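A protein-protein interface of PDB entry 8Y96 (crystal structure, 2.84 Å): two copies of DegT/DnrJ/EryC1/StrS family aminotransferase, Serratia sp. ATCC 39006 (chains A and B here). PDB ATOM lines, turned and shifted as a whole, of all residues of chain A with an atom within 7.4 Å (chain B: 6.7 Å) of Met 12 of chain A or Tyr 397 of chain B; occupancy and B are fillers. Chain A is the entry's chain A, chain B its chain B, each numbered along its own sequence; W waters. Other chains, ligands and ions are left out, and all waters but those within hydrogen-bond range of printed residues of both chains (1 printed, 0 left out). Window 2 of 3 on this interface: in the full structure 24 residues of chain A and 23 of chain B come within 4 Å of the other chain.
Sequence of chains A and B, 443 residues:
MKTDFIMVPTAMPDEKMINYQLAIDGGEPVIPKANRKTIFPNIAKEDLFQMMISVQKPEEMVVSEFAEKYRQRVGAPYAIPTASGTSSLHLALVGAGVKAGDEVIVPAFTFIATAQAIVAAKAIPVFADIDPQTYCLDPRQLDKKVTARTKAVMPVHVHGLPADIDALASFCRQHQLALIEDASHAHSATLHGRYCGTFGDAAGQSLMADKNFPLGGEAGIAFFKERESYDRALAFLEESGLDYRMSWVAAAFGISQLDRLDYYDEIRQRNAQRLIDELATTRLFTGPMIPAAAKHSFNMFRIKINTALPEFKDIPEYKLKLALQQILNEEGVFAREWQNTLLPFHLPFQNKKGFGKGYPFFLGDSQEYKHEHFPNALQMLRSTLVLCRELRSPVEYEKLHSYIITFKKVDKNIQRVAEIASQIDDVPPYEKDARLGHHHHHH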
ATOM      1  N   PRO A   9     -26.685  16.696  14.560  1.00  0.00           N
ATOM      2  CA  PRO A   9     -25.269  16.515  14.882  1.00  0.00           C
ATOM      3  C   PRO A   9     -25.107  15.377  15.883  1.00  0.00           C
ATOM      4  O   PRO A   9     -26.016  15.112  16.664  1.00  0.00           O
ATOM      5  CB  PRO A   9     -24.831  17.870  15.455  1.00  0.00           C
ATOM      6  CG  PRO A   9     -26.103  18.470  16.013  1.00  0.00           C
ATOM      7  CD  PRO A   9     -27.256  17.894  15.197  1.00  0.00           C
ATOM      8  N   THR A  10     -23.947  14.712  15.834  1.00  0.00           N
ATOM      9  CA  THR A  10     -23.632  13.631  16.752  1.00  0.00           C
ATOM     10  C   THR A  10     -23.258  14.240  18.101  1.00  0.00           C
ATOM     11  O   THR A  10     -22.365  15.080  18.178  1.00  0.00           O
ATOM     12  CB  THR A  10     -22.494  12.777  16.192  1.00  0.00           C
ATOM     13  OG1 THR A  10     -22.773  12.571  14.811  1.00  0.00           O
ATOM     14  CG2 THR A  10     -22.369  11.439  16.901  1.00  0.00           C
ATOM     15  N   ALA A  11     -23.959  13.819  19.158  1.00  0.00           N
ATOM     16  CA  ALA A  11     -23.658  14.286  20.501  1.00  0.00           C
ATOM     17  C   ALA A  11     -22.314  13.711  20.939  1.00  0.00           C
ATOM     18  O   ALA A  11     -21.922  12.633  20.501  1.00  0.00           O
ATOM     19  CB  ALA A  11     -24.764  13.893  21.458  1.00  0.00           C
ATOM     20  N   MET A  12     -21.603  14.454  21.790  1.00  0.00           N
ATOM     21  CA  MET A  12     -20.454  13.888  22.466  1.00  0.00           C
ATOM     22  C   MET A  12     -20.978  12.796  23.396  1.00  0.00           C
ATOM     23  O   MET A  12     -21.721  13.092  24.331  1.00  0.00           O
ATOM     24  CB  MET A  12     -19.674  14.958  23.241  1.00  0.00           C
ATOM     25  CG  MET A  12     -18.320  14.480  23.730  1.00  0.00           C
ATOM     26  SD  MET A  12     -17.161  14.171  22.381  1.00  0.00           S
ATOM     27  CE  MET A  12     -16.229  12.803  23.085  1.00  0.00           C
ATOM     28  N   PRO A  13     -20.655  11.504  23.148  1.00  0.00           N
ATOM     29  CA  PRO A  13     -21.229  10.404  23.926  1.00  0.00           C
ATOM     30  C   PRO A  13     -20.603  10.286  25.309  1.00  0.00           C
ATOM     31  O   PRO A  13     -19.430  10.595  25.492  1.00  0.00           O
ATOM     32  CB  PRO A  13     -20.917   9.181  23.057  1.00  0.00           C
ATOM     33  CG  PRO A  13     -19.597   9.538  22.413  1.00  0.00           C
ATOM     34  CD  PRO A  13     -19.703  11.032  22.126  1.00  0.00           C
ATOM     35  N   ASP A  14     -21.401   9.816  26.270  1.00  0.00           N
ATOM     36  CA  ASP A  14     -20.938   9.625  27.633  1.00  0.00           C
ATOM     37  C   ASP A  14     -19.992   8.425  27.665  1.00  0.00           C
ATOM     38  O   ASP A  14     -20.368   7.325  27.265  1.00  0.00           O
ATOM     39  CB  ASP A  14     -22.120   9.448  28.572  1.00  0.00           C
ATOM     40  CG  ASP A  14     -21.834   9.689  30.045  1.00  0.00           C
ATOM     41  OD1 ASP A  14     -20.667  10.003  30.373  1.00  0.00           O
ATOM     42  OD2 ASP A  14     -22.787   9.574  30.846  1.00  0.00           O
ATOM     43  N   GLU A  15     -18.765   8.640  28.155  1.00  0.00           N
ATOM     44  CA  GLU A  15     -17.775   7.576  28.250  1.00  0.00           C
ATOM     45  C   GLU A  15     -18.281   6.495  29.205  1.00  0.00           C
ATOM     46  O   GLU A  15     -17.797   5.366  29.183  1.00  0.00           O
ATOM     47  CB  GLU A  15     -16.414   8.139  28.669  1.00  0.00           C
ATOM     48  CG  GLU A  15     -15.273   7.130  28.550  1.00  0.00           C
ATOM     49  CD  GLU A  15     -13.886   7.741  28.417  1.00  0.00           C
ATOM     50  OE1 GLU A  15     -13.456   8.467  29.343  1.00  0.00           O
ATOM     51  OE2 GLU A  15     -13.232   7.486  27.381  1.00  0.00           O
ATOM     52  N   MET A  17     -20.964   5.063  28.884  1.00  0.00           N
ATOM     53  CA  MET A  17     -21.729   4.103  28.101  1.00  0.00           C
ATOM     54  C   MET A  17     -20.971   2.784  27.958  1.00  0.00           C
ATOM     55  O   MET A  17     -21.553   1.793  27.525  1.00  0.00           O
ATOM     56  CB  MET A  17     -22.069   4.626  26.699  1.00  0.00           C
ATOM     57  CG  MET A  17     -23.173   5.670  26.671  1.00  0.00           C
ATOM     58  SD  MET A  17     -24.069   5.706  25.106  1.00  0.00           S
ATOM     59  CE  MET A  17     -24.235   7.483  24.879  1.00  0.00           C
ATOM     60  N   GLU A 396     -16.331  13.482  12.002  1.00  0.00           N
ATOM     61  CA  GLU A 396     -16.085  14.465  13.045  1.00  0.00           C
ATOM     62  C   GLU A 396     -15.698  13.734  14.329  1.00  0.00           C
ATOM     63  O   GLU A 396     -15.913  12.530  14.449  1.00  0.00           O
ATOM     64  CB  GLU A 396     -17.292  15.398  13.195  1.00  0.00           C
ATOM     65  CG  GLU A 396     -18.569  14.766  13.759  1.00  0.00           C
ATOM     66  CD  GLU A 396     -19.490  14.004  12.809  1.00  0.00           C
ATOM     67  OE1 GLU A 396     -19.084  13.663  11.671  1.00  0.00           O
ATOM     68  OE2 GLU A 396     -20.653  13.762  13.221  1.00  0.00           O
ATOM     69  N   TYR A 397     -15.126  14.481  15.281  1.00  0.00           N
ATOM     70  CA  TYR A 397     -14.504  13.919  16.472  1.00  0.00           C
ATOM     71  C   TYR A 397     -15.513  13.110  17.283  1.00  0.00           C
ATOM     72  O   TYR A 397     -15.207  12.005  17.726  1.00  0.00           O
ATOM     73  CB  TYR A 397     -13.904  15.063  17.294  1.00  0.00           C
ATOM     74  CG  TYR A 397     -13.317  14.633  18.630  1.00  0.00           C
ATOM     75  CD1 TYR A 397     -14.097  14.604  19.782  1.00  0.00           C
ATOM     76  CD2 TYR A 397     -11.983  14.251  18.740  1.00  0.00           C
ATOM     77  CE1 TYR A 397     -13.572  14.205  20.999  1.00  0.00           C
ATOM     78  CE2 TYR A 397     -11.446  13.853  19.953  1.00  0.00           C
ATOM     79  CZ  TYR A 397     -12.241  13.834  21.086  1.00  0.00           C
ATOM     80  OH  TYR A 397     -11.714  13.445  22.284  1.00  0.00           O
ATOM     81  N   GLU A 398     -16.707  13.680  17.480  1.00  0.00           N
ATOM     82  CA  GLU A 398     -17.775  13.042  18.232  1.00  0.00           C
ATOM     83  C   GLU A 398     -18.075  11.649  17.672  1.00  0.00           C
ATOM     84  O   GLU A 398     -18.283  10.701  18.428  1.00  0.00           O
ATOM     85  CB  GLU A 398     -19.039  13.902  18.194  1.00  0.00           C
ATOM     86  CG  GLU A 398     -18.942  15.211  18.975  1.00  0.00           C
ATOM     87  CD  GLU A 398     -18.436  16.440  18.235  1.00  0.00           C
ATOM     88  OE1 GLU A 398     -17.965  16.353  17.081  1.00  0.00           O
ATOM     89  OE2 GLU A 398     -18.535  17.524  18.841  1.00  0.00           O
ATOM     90  N   LYS A 399     -18.110  11.532  16.341  1.00  0.00           N
ATOM     91  CA  LYS A 399     -18.418  10.270  15.689  1.00  0.00           C
ATOM     92  C   LYS A 399     -17.294   9.265  15.929  1.00  0.00           C
ATOM     93  O   LYS A 399     -17.557   8.079  16.105  1.00  0.00           O
ATOM     94  CB  LYS A 399     -18.619  10.483  14.184  1.00  0.00           C
ATOM     95  CG  LYS A 399     -19.174   9.291  13.423  1.00  0.00           C
ATOM     96  CD  LYS A 399     -20.466   8.756  14.029  1.00  0.00           C
ATOM     97  CE  LYS A 399     -21.306   8.007  13.050  1.00  0.00           C
ATOM     98  NZ  LYS A 399     -22.006   8.924  12.148  1.00  0.00           N
ATOM     99  N   LEU A 400     -16.046   9.753  15.926  1.00  0.00           N
ATOM    100  CA  LEU A 400     -14.879   8.901  16.087  1.00  0.00           C
ATOM    101  C   LEU A 400     -14.851   8.299  17.491  1.00  0.00           C
ATOM    102  O   LEU A 400     -14.557   7.116  17.651  1.00  0.00           O
ATOM    103  CB  LEU A 400     -13.611   9.702  15.800  1.00  0.00           C
ATOM    104  CG  LEU A 400     -12.291   9.000  16.136  1.00  0.00           C
ATOM    105  CD1 LEU A 400     -12.084   7.784  15.248  1.00  0.00           C
ATOM    106  CD2 LEU A 400     -11.131   9.970  16.026  1.00  0.00           C
ATOM    107  N   HIS A 401     -15.136   9.126  18.503  1.00  0.00           N
ATOM    108  CA  HIS A 401     -15.141   8.678  19.887  1.00  0.00           C
ATOM    109  C   HIS A 401     -16.290   7.701  20.124  1.00  0.00           C
ATOM    110  O   HIS A 401     -16.191   6.832  20.991  1.00  0.00           O
ATOM    111  CB  HIS A 401     -15.129   9.872  20.848  1.00  0.00           C
ATOM    112  CG  HIS A 401     -13.739  10.291  21.189  1.00  0.00           C
ATOM    113  ND1 HIS A 401     -13.187  10.079  22.436  1.00  0.00           N
ATOM    114  CD2 HIS A 401     -12.782  10.878  20.449  1.00  0.00           C
ATOM    115  CE1 HIS A 401     -11.938  10.532  22.438  1.00  0.00           C
ATOM    116  NE2 HIS A 401     -11.670  11.018  21.239  1.00  0.00           N
ATOM    117  N   SER A 402     -17.367   7.845  19.342  1.00  0.00           N
ATOM    118  CA  SER A 402     -18.476   6.908  19.396  1.00  0.00           C
ATOM    119  C   SER A 402     -18.015   5.524  18.942  1.00  0.00           C
ATOM    120  O   SER A 402     -18.429   4.520  19.515  1.00  0.00           O
ATOM    121  CB  SER A 402     -19.658   7.404  18.602  1.00  0.00           C
ATOM    122  OG  SER A 402     -20.169   8.614  19.146  1.00  0.00           O
ATOM    123  N   ILE A 405     -15.906   4.241  21.874  1.00  0.00           N
ATOM    124  CA  ILE A 405     -16.752   3.807  22.975  1.00  0.00           C
ATOM    125  C   ILE A 405     -17.358   2.448  22.642  1.00  0.00           C
ATOM    126  O   ILE A 405     -17.450   1.592  23.515  1.00  0.00           O
ATOM    127  CB  ILE A 405     -17.845   4.848  23.291  1.00  0.00           C
ATOM    128  CG1 ILE A 405     -17.259   6.121  23.900  1.00  0.00           C
ATOM    129  CG2 ILE A 405     -18.930   4.256  24.190  1.00  0.00           C
ATOM    130  CD1 ILE A 405     -16.567   5.906  25.234  1.00  0.00           C
ATOM    131  N   MET B  12      -6.351  18.286  17.492  1.00  0.00           N
ATOM    132  CA  MET B  12      -6.792  18.209  18.871  1.00  0.00           C
ATOM    133  C   MET B  12      -5.703  18.810  19.755  1.00  0.00           C
ATOM    134  O   MET B  12      -4.577  18.322  19.756  1.00  0.00           O
ATOM    135  CB  MET B  12      -7.039  16.749  19.267  1.00  0.00           C
ATOM    136  CG  MET B  12      -7.709  16.594  20.611  1.00  0.00           C
ATOM    137  SD  MET B  12      -9.399  17.219  20.573  1.00  0.00           S
ATOM    138  CE  MET B  12      -9.558  17.718  22.293  1.00  0.00           C
ATOM    139  N   PRO B  13      -5.986  19.876  20.536  1.00  0.00           N
ATOM    140  CA  PRO B  13      -4.948  20.526  21.336  1.00  0.00           C
ATOM    141  C   PRO B  13      -4.562  19.657  22.528  1.00  0.00           C
ATOM    142  O   PRO B  13      -5.426  19.012  23.124  1.00  0.00           O
ATOM    143  CB  PRO B  13      -5.625  21.837  21.761  1.00  0.00           C
ATOM    144  CG  PRO B  13      -7.084  21.454  21.882  1.00  0.00           C
ATOM    145  CD  PRO B  13      -7.315  20.477  20.735  1.00  0.00           C
ATOM    146  N   ARG B 270     -24.733  23.711  22.005  1.00  0.00           N
ATOM    147  CA  ARG B 270     -23.904  22.766  22.739  1.00  0.00           C
ATOM    148  C   ARG B 270     -22.490  23.314  22.914  1.00  0.00           C
ATOM    149  O   ARG B 270     -21.900  23.137  23.975  1.00  0.00           O
ATOM    150  CB  ARG B 270     -23.844  21.386  22.075  1.00  0.00           C
ATOM    151  CG  ARG B 270     -25.144  20.600  22.149  1.00  0.00           C
ATOM    152  CD  ARG B 270     -24.901  19.112  21.915  1.00  0.00           C
ATOM    153  NE  ARG B 270     -26.082  18.412  21.391  1.00  0.00           N
ATOM    154  CZ  ARG B 270     -26.152  17.686  20.269  1.00  0.00           C
ATOM    155  NH1 ARG B 270     -25.078  17.460  19.525  1.00  0.00           N
ATOM    156  NH2 ARG B 270     -27.310  17.166  19.898  1.00  0.00           N
ATOM    157  N   ASN B 271     -21.951  23.969  21.878  1.00  0.00           N
ATOM    158  CA  ASN B 271     -20.620  24.557  21.952  1.00  0.00           C
ATOM    159  C   ASN B 271     -20.591  25.653  23.018  1.00  0.00           C
ATOM    160  O   ASN B 271     -19.765  25.613  23.926  1.00  0.00           O
ATOM    161  CB  ASN B 271     -20.152  25.103  20.605  1.00  0.00           C
ATOM    162  CG  ASN B 271     -19.684  24.025  19.655  1.00  0.00           C
ATOM    163  OD1 ASN B 271     -19.795  22.829  19.952  1.00  0.00           O
ATOM    164  ND2 ASN B 271     -19.155  24.425  18.508  1.00  0.00           N
ATOM    165  N   ARG B 274     -20.979  24.356  26.642  1.00  0.00           N
ATOM    166  CA  ARG B 274     -19.779  23.719  27.158  1.00  0.00           C
ATOM    167  C   ARG B 274     -18.792  24.786  27.630  1.00  0.00           C
ATOM    168  O   ARG B 274     -18.148  24.624  28.664  1.00  0.00           O
ATOM    169  CB  ARG B 274     -19.166  22.804  26.095  1.00  0.00           C
ATOM    170  CG  ARG B 274     -17.988  21.957  26.559  1.00  0.00           C
ATOM    171  CD  ARG B 274     -18.291  21.088  27.778  1.00  0.00           C
ATOM    172  NE  ARG B 274     -17.576  19.805  27.745  1.00  0.00           N
ATOM    173  CZ  ARG B 274     -16.265  19.604  27.886  1.00  0.00           C
ATOM    174  NH1 ARG B 274     -15.464  20.588  28.254  1.00  0.00           N
ATOM    175  NH2 ARG B 274     -15.758  18.400  27.684  1.00  0.00           N
ATOM    176  N   VAL B 395     -18.366  25.674  15.110  1.00  0.00           N
ATOM    177  CA  VAL B 395     -17.017  25.146  14.984  1.00  0.00           C
ATOM    178  C   VAL B 395     -16.984  23.714  15.515  1.00  0.00           C
ATOM    179  O   VAL B 395     -17.839  23.315  16.301  1.00  0.00           O
ATOM    180  CB  VAL B 395     -15.979  26.044  15.693  1.00  0.00           C
ATOM    181  CG1 VAL B 395     -16.018  27.478  15.179  1.00  0.00           C
ATOM    182  CG2 VAL B 395     -16.128  26.028  17.212  1.00  0.00           C
ATOM    183  N   GLU B 396     -15.968  22.962  15.077  1.00  0.00           N
ATOM    184  CA  GLU B 396     -15.783  21.567  15.446  1.00  0.00           C
ATOM    185  C   GLU B 396     -15.244  21.462  16.874  1.00  0.00           C
ATOM    186  O   GLU B 396     -14.806  22.450  17.455  1.00  0.00           O
ATOM    187  CB  GLU B 396     -14.872  20.895  14.415  1.00  0.00           C
ATOM    188  CG  GLU B 396     -13.419  21.373  14.430  1.00  0.00           C
ATOM    189  CD  GLU B 396     -13.055  22.581  13.578  1.00  0.00           C
ATOM    190  OE1 GLU B 396     -13.803  23.588  13.561  1.00  0.00           O
ATOM    191  OE2 GLU B 396     -11.973  22.515  12.947  1.00  0.00           O
ATOM    192  N   TYR B 397     -15.261  20.239  17.420  1.00  0.00           N
ATOM    193  CA  TYR B 397     -14.878  19.958  18.797  1.00  0.00           C
ATOM    194  C   TYR B 397     -13.458  20.447  19.076  1.00  0.00           C
ATOM    195  O   TYR B 397     -13.191  20.999  20.143  1.00  0.00           O
ATOM    196  CB  TYR B 397     -14.997  18.449  19.029  1.00  0.00           C
ATOM    197  CG  TYR B 397     -14.724  17.965  20.446  1.00  0.00           C
ATOM    198  CD1 TYR B 397     -13.427  17.760  20.905  1.00  0.00           C
ATOM    199  CD2 TYR B 397     -15.770  17.682  21.317  1.00  0.00           C
ATOM    200  CE1 TYR B 397     -13.178  17.312  22.193  1.00  0.00           C
ATOM    201  CE2 TYR B 397     -15.534  17.226  22.606  1.00  0.00           C
ATOM    202  CZ  TYR B 397     -14.234  17.039  23.044  1.00  0.00           C
ATOM    203  OH  TYR B 397     -14.001  16.599  24.317  1.00  0.00           O
ATOM    204  N   GLU B 398     -12.559  20.223  18.108  1.00  0.00           N
ATOM    205  CA  GLU B 398     -11.147  20.553  18.233  1.00  0.00           C
ATOM    206  C   GLU B 398     -10.965  22.056  18.457  1.00  0.00           C
ATOM    207  O   GLU B 398     -10.110  22.470  19.239  1.00  0.00           O
ATOM    208  CB  GLU B 398     -10.390  20.062  16.996  1.00  0.00           C
ATOM    209  CG  GLU B 398     -10.370  18.540  16.841  1.00  0.00           C
ATOM    210  CD  GLU B 398     -11.456  17.913  15.973  1.00  0.00           C
ATOM    211  OE1 GLU B 398     -12.594  18.433  15.932  1.00  0.00           O
ATOM    212  OE2 GLU B 398     -11.168  16.862  15.358  1.00  0.00           O
ATOM    213  N   LYS B 399     -11.781  22.866  17.770  1.00  0.00           N
ATOM    214  CA  LYS B 399     -11.712  24.315  17.867  1.00  0.00           C
ATOM    215  C   LYS B 399     -12.282  24.785  19.204  1.00  0.00           C
ATOM    216  O   LYS B 399     -11.759  25.709  19.819  1.00  0.00           O
ATOM    217  CB  LYS B 399     -12.505  24.962  16.728  1.00  0.00           C
ATOM    218  CG  LYS B 399     -12.153  26.415  16.445  1.00  0.00           C
ATOM    219  CD  LYS B 399     -10.711  26.596  15.976  1.00  0.00           C
ATOM    220  CE  LYS B 399     -10.431  27.967  15.462  1.00  0.00           C
ATOM    221  NZ  LYS B 399     -11.030  28.197  14.147  1.00  0.00           N
ATOM    222  N   LEU B 400     -13.379  24.160  19.635  1.00  0.00           N
ATOM    223  CA  LEU B 400     -14.040  24.558  20.866  1.00  0.00           C
ATOM    224  C   LEU B 400     -13.119  24.292  22.051  1.00  0.00           C
ATOM    225  O   LEU B 400     -13.004  25.129  22.947  1.00  0.00           O
ATOM    226  CB  LEU B 400     -15.364  23.819  21.035  1.00  0.00           C
ATOM    227  CG  LEU B 400     -16.167  24.186  22.285  1.00  0.00           C
ATOM    228  CD1 LEU B 400     -16.719  25.594  22.167  1.00  0.00           C
ATOM    229  CD2 LEU B 400     -17.271  23.178  22.516  1.00  0.00           C
ATOM    230  N   HIS B 401     -12.479  23.119  22.049  1.00  0.00           N
ATOM    231  CA  HIS B 401     -11.559  22.745  23.108  1.00  0.00           C
ATOM    232  C   HIS B 401     -10.347  23.673  23.074  1.00  0.00           C
ATOM    233  O   HIS B 401      -9.849  24.071  24.125  1.00  0.00           O
ATOM    234  CB  HIS B 401     -11.297  21.235  23.051  1.00  0.00           C
ATOM    235  CG  HIS B 401     -12.415  20.475  23.681  1.00  0.00           C
ATOM    236  ND1 HIS B 401     -13.693  20.497  23.168  1.00  0.00           N
ATOM    237  CD2 HIS B 401     -12.481  19.757  24.807  1.00  0.00           C
ATOM    238  CE1 HIS B 401     -14.490  19.787  23.950  1.00  0.00           C
ATOM    239  NE2 HIS B 401     -13.773  19.320  24.947  1.00  0.00           N
ATOM    240  N   SER B 402      -9.913  24.052  21.864  1.00  0.00           N
ATOM    241  CA  SER B 402      -8.862  25.044  21.695  1.00  0.00           C
ATOM    242  C   SER B 402      -9.214  26.339  22.429  1.00  0.00           C
ATOM    243  O   SER B 402      -8.355  26.926  23.080  1.00  0.00           O
ATOM    244  CB  SER B 402      -8.564  25.309  20.242  1.00  0.00           C
ATOM    245  OG  SER B 402      -7.929  24.187  19.642  1.00  0.00           O
ATOM    246  N   ILE B 404     -11.296  26.537  25.029  1.00  0.00           N
ATOM    247  CA  ILE B 404     -11.318  26.213  26.449  1.00  0.00           C
ATOM    248  C   ILE B 404      -9.893  26.239  27.004  1.00  0.00           C
ATOM    249  O   ILE B 404      -9.647  26.847  28.043  1.00  0.00           O
ATOM    250  CB  ILE B 404     -12.014  24.861  26.706  1.00  0.00           C
ATOM    251  CG1 ILE B 404     -13.467  24.868  26.207  1.00  0.00           C
ATOM    252  CG2 ILE B 404     -11.937  24.478  28.187  1.00  0.00           C
ATOM    253  CD1 ILE B 404     -14.113  23.495  26.126  1.00  0.00           C
HETATM  254  O   HOH W   1     -14.622  17.251  14.559  1.00  0.00           O
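Of the printed residues of chain B, Ala 11 of chain A touches Arg 270 (3.6 Å).
Met 12 of chain A touches just one residue of chain B: Tyr 397.
Of the printed residues of chain B, Tyr 397 of chain A touches Met 12 (3.99 Å), Tyr 397 (3.4 Å) and Glu 398 (3.8 Å).
Of the printed residues of chain B, Glu 398 of chain A touches Tyr 397.
Of the printed residues of chain A, Met 12 of chain B touches Tyr 397 (3.99 Å).
Of the printed residues of chain A, Arg 270 of chain B touches Pro 9 (3.8 Å), Thr 10 (3.9 Å) and Ala 11 (3.6 Å).
Tyr 397 of chain B touches three residues of chain A.
His 401 of chain B touches none of the printed residues of chain A.
The nearest residue of chain B that does not touch Met 12 of chain A is Arg 270 of chain B (5.1 Å).
The nearest residue of chain A that does not touch Tyr 397 of chain B is His 401 of chain A (6.5 Å).
The nearest printed residue of chain A that does not touch Arg 270 of chain B is Met 12 of chain A (5.1 Å).
Met 12 of chain A touches Tyr 397 of chain B, and with the chains exchanged Tyr 397 of chain A touches Met 12 of chain B.
Tyr 397 of chain B touches its own counterpart, Tyr 397 of chain A.
Tyr 397 of chain A touches Glu 398 of chain B, and with the chains exchanged Glu 398 of chain A touches Tyr 397 of chain B.
Positions printed for both chains: 12, 13, 396, 397, 398, 399, 400, 401 and 402.
Of the 8 pairs that touch across the chains among the printed residues, 5 have their exchanged pair printed and touching as well.
Of the 14 printed residues of chain B, 4 touch a printed residue of chain A.
Hydrophobic or aromatic side chains of chain B that line the printed part of chain A: Met 12 and Tyr 397.
Of the 16 printed residues of chain A, 6 touch a printed residue of chain B.
NH1 of Arg 270 of chain B touches CG of Pro 9 of chain A, at 3.8 Å.
Arg 270 of chain B touches Thr 10 of chain A (NH1 to O, 3.9 Å).
NH1 of Arg 270 of chain B touches CA of Ala 11 of chain A, at 3.6 Å.
Tyr 397 of chain B touches Met 12 of chain A.
Tyr 397 of chain A touches Met 12 of chain B.
CE1 of Tyr 397 of chain B touches CE1 of Tyr 397 of chain A, at 3.4 Å.
Glu 398 of chain B touches Tyr 397 of chain A (OE2 to CB, 3.8 Å).
Glu 398 of chain A touches Tyr 397 of chain B (OE2 to CB, 3.7 Å).
Water W1 lies within hydrogen-bond range of OE1 of Glu 398 of chain B and N of Tyr 397 of chain A.
OH of Tyr 397 of chain B sits at hydrogen-bond distance from NE2 of His 401 of chain B.
The side-chain hydroxyl of Ser 402 of chain B sits at hydrogen-bond distance from the backbone carbonyl oxygen of Glu 398 of chain B, 2.8 Å away.
The side-chain hydroxyl of Tyr 397 of chain A sits at hydrogen-bond distance from a ring nitrogen (NE2) of His 401 of chain A, at 2.6 Å.
The side-chain hydroxyl (OG1) of Thr 10 of chain A sits at hydrogen-bond distance from the side-chain carboxylate (OE2) of Glu 396 of chain A (2.9 Å).
The side-chain hydroxyl (OG) of Ser 402 of chain A lies within hydrogen-bond range of the backbone carbonyl oxygen (O) of Glu 398 of chain A (2.9 Å).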
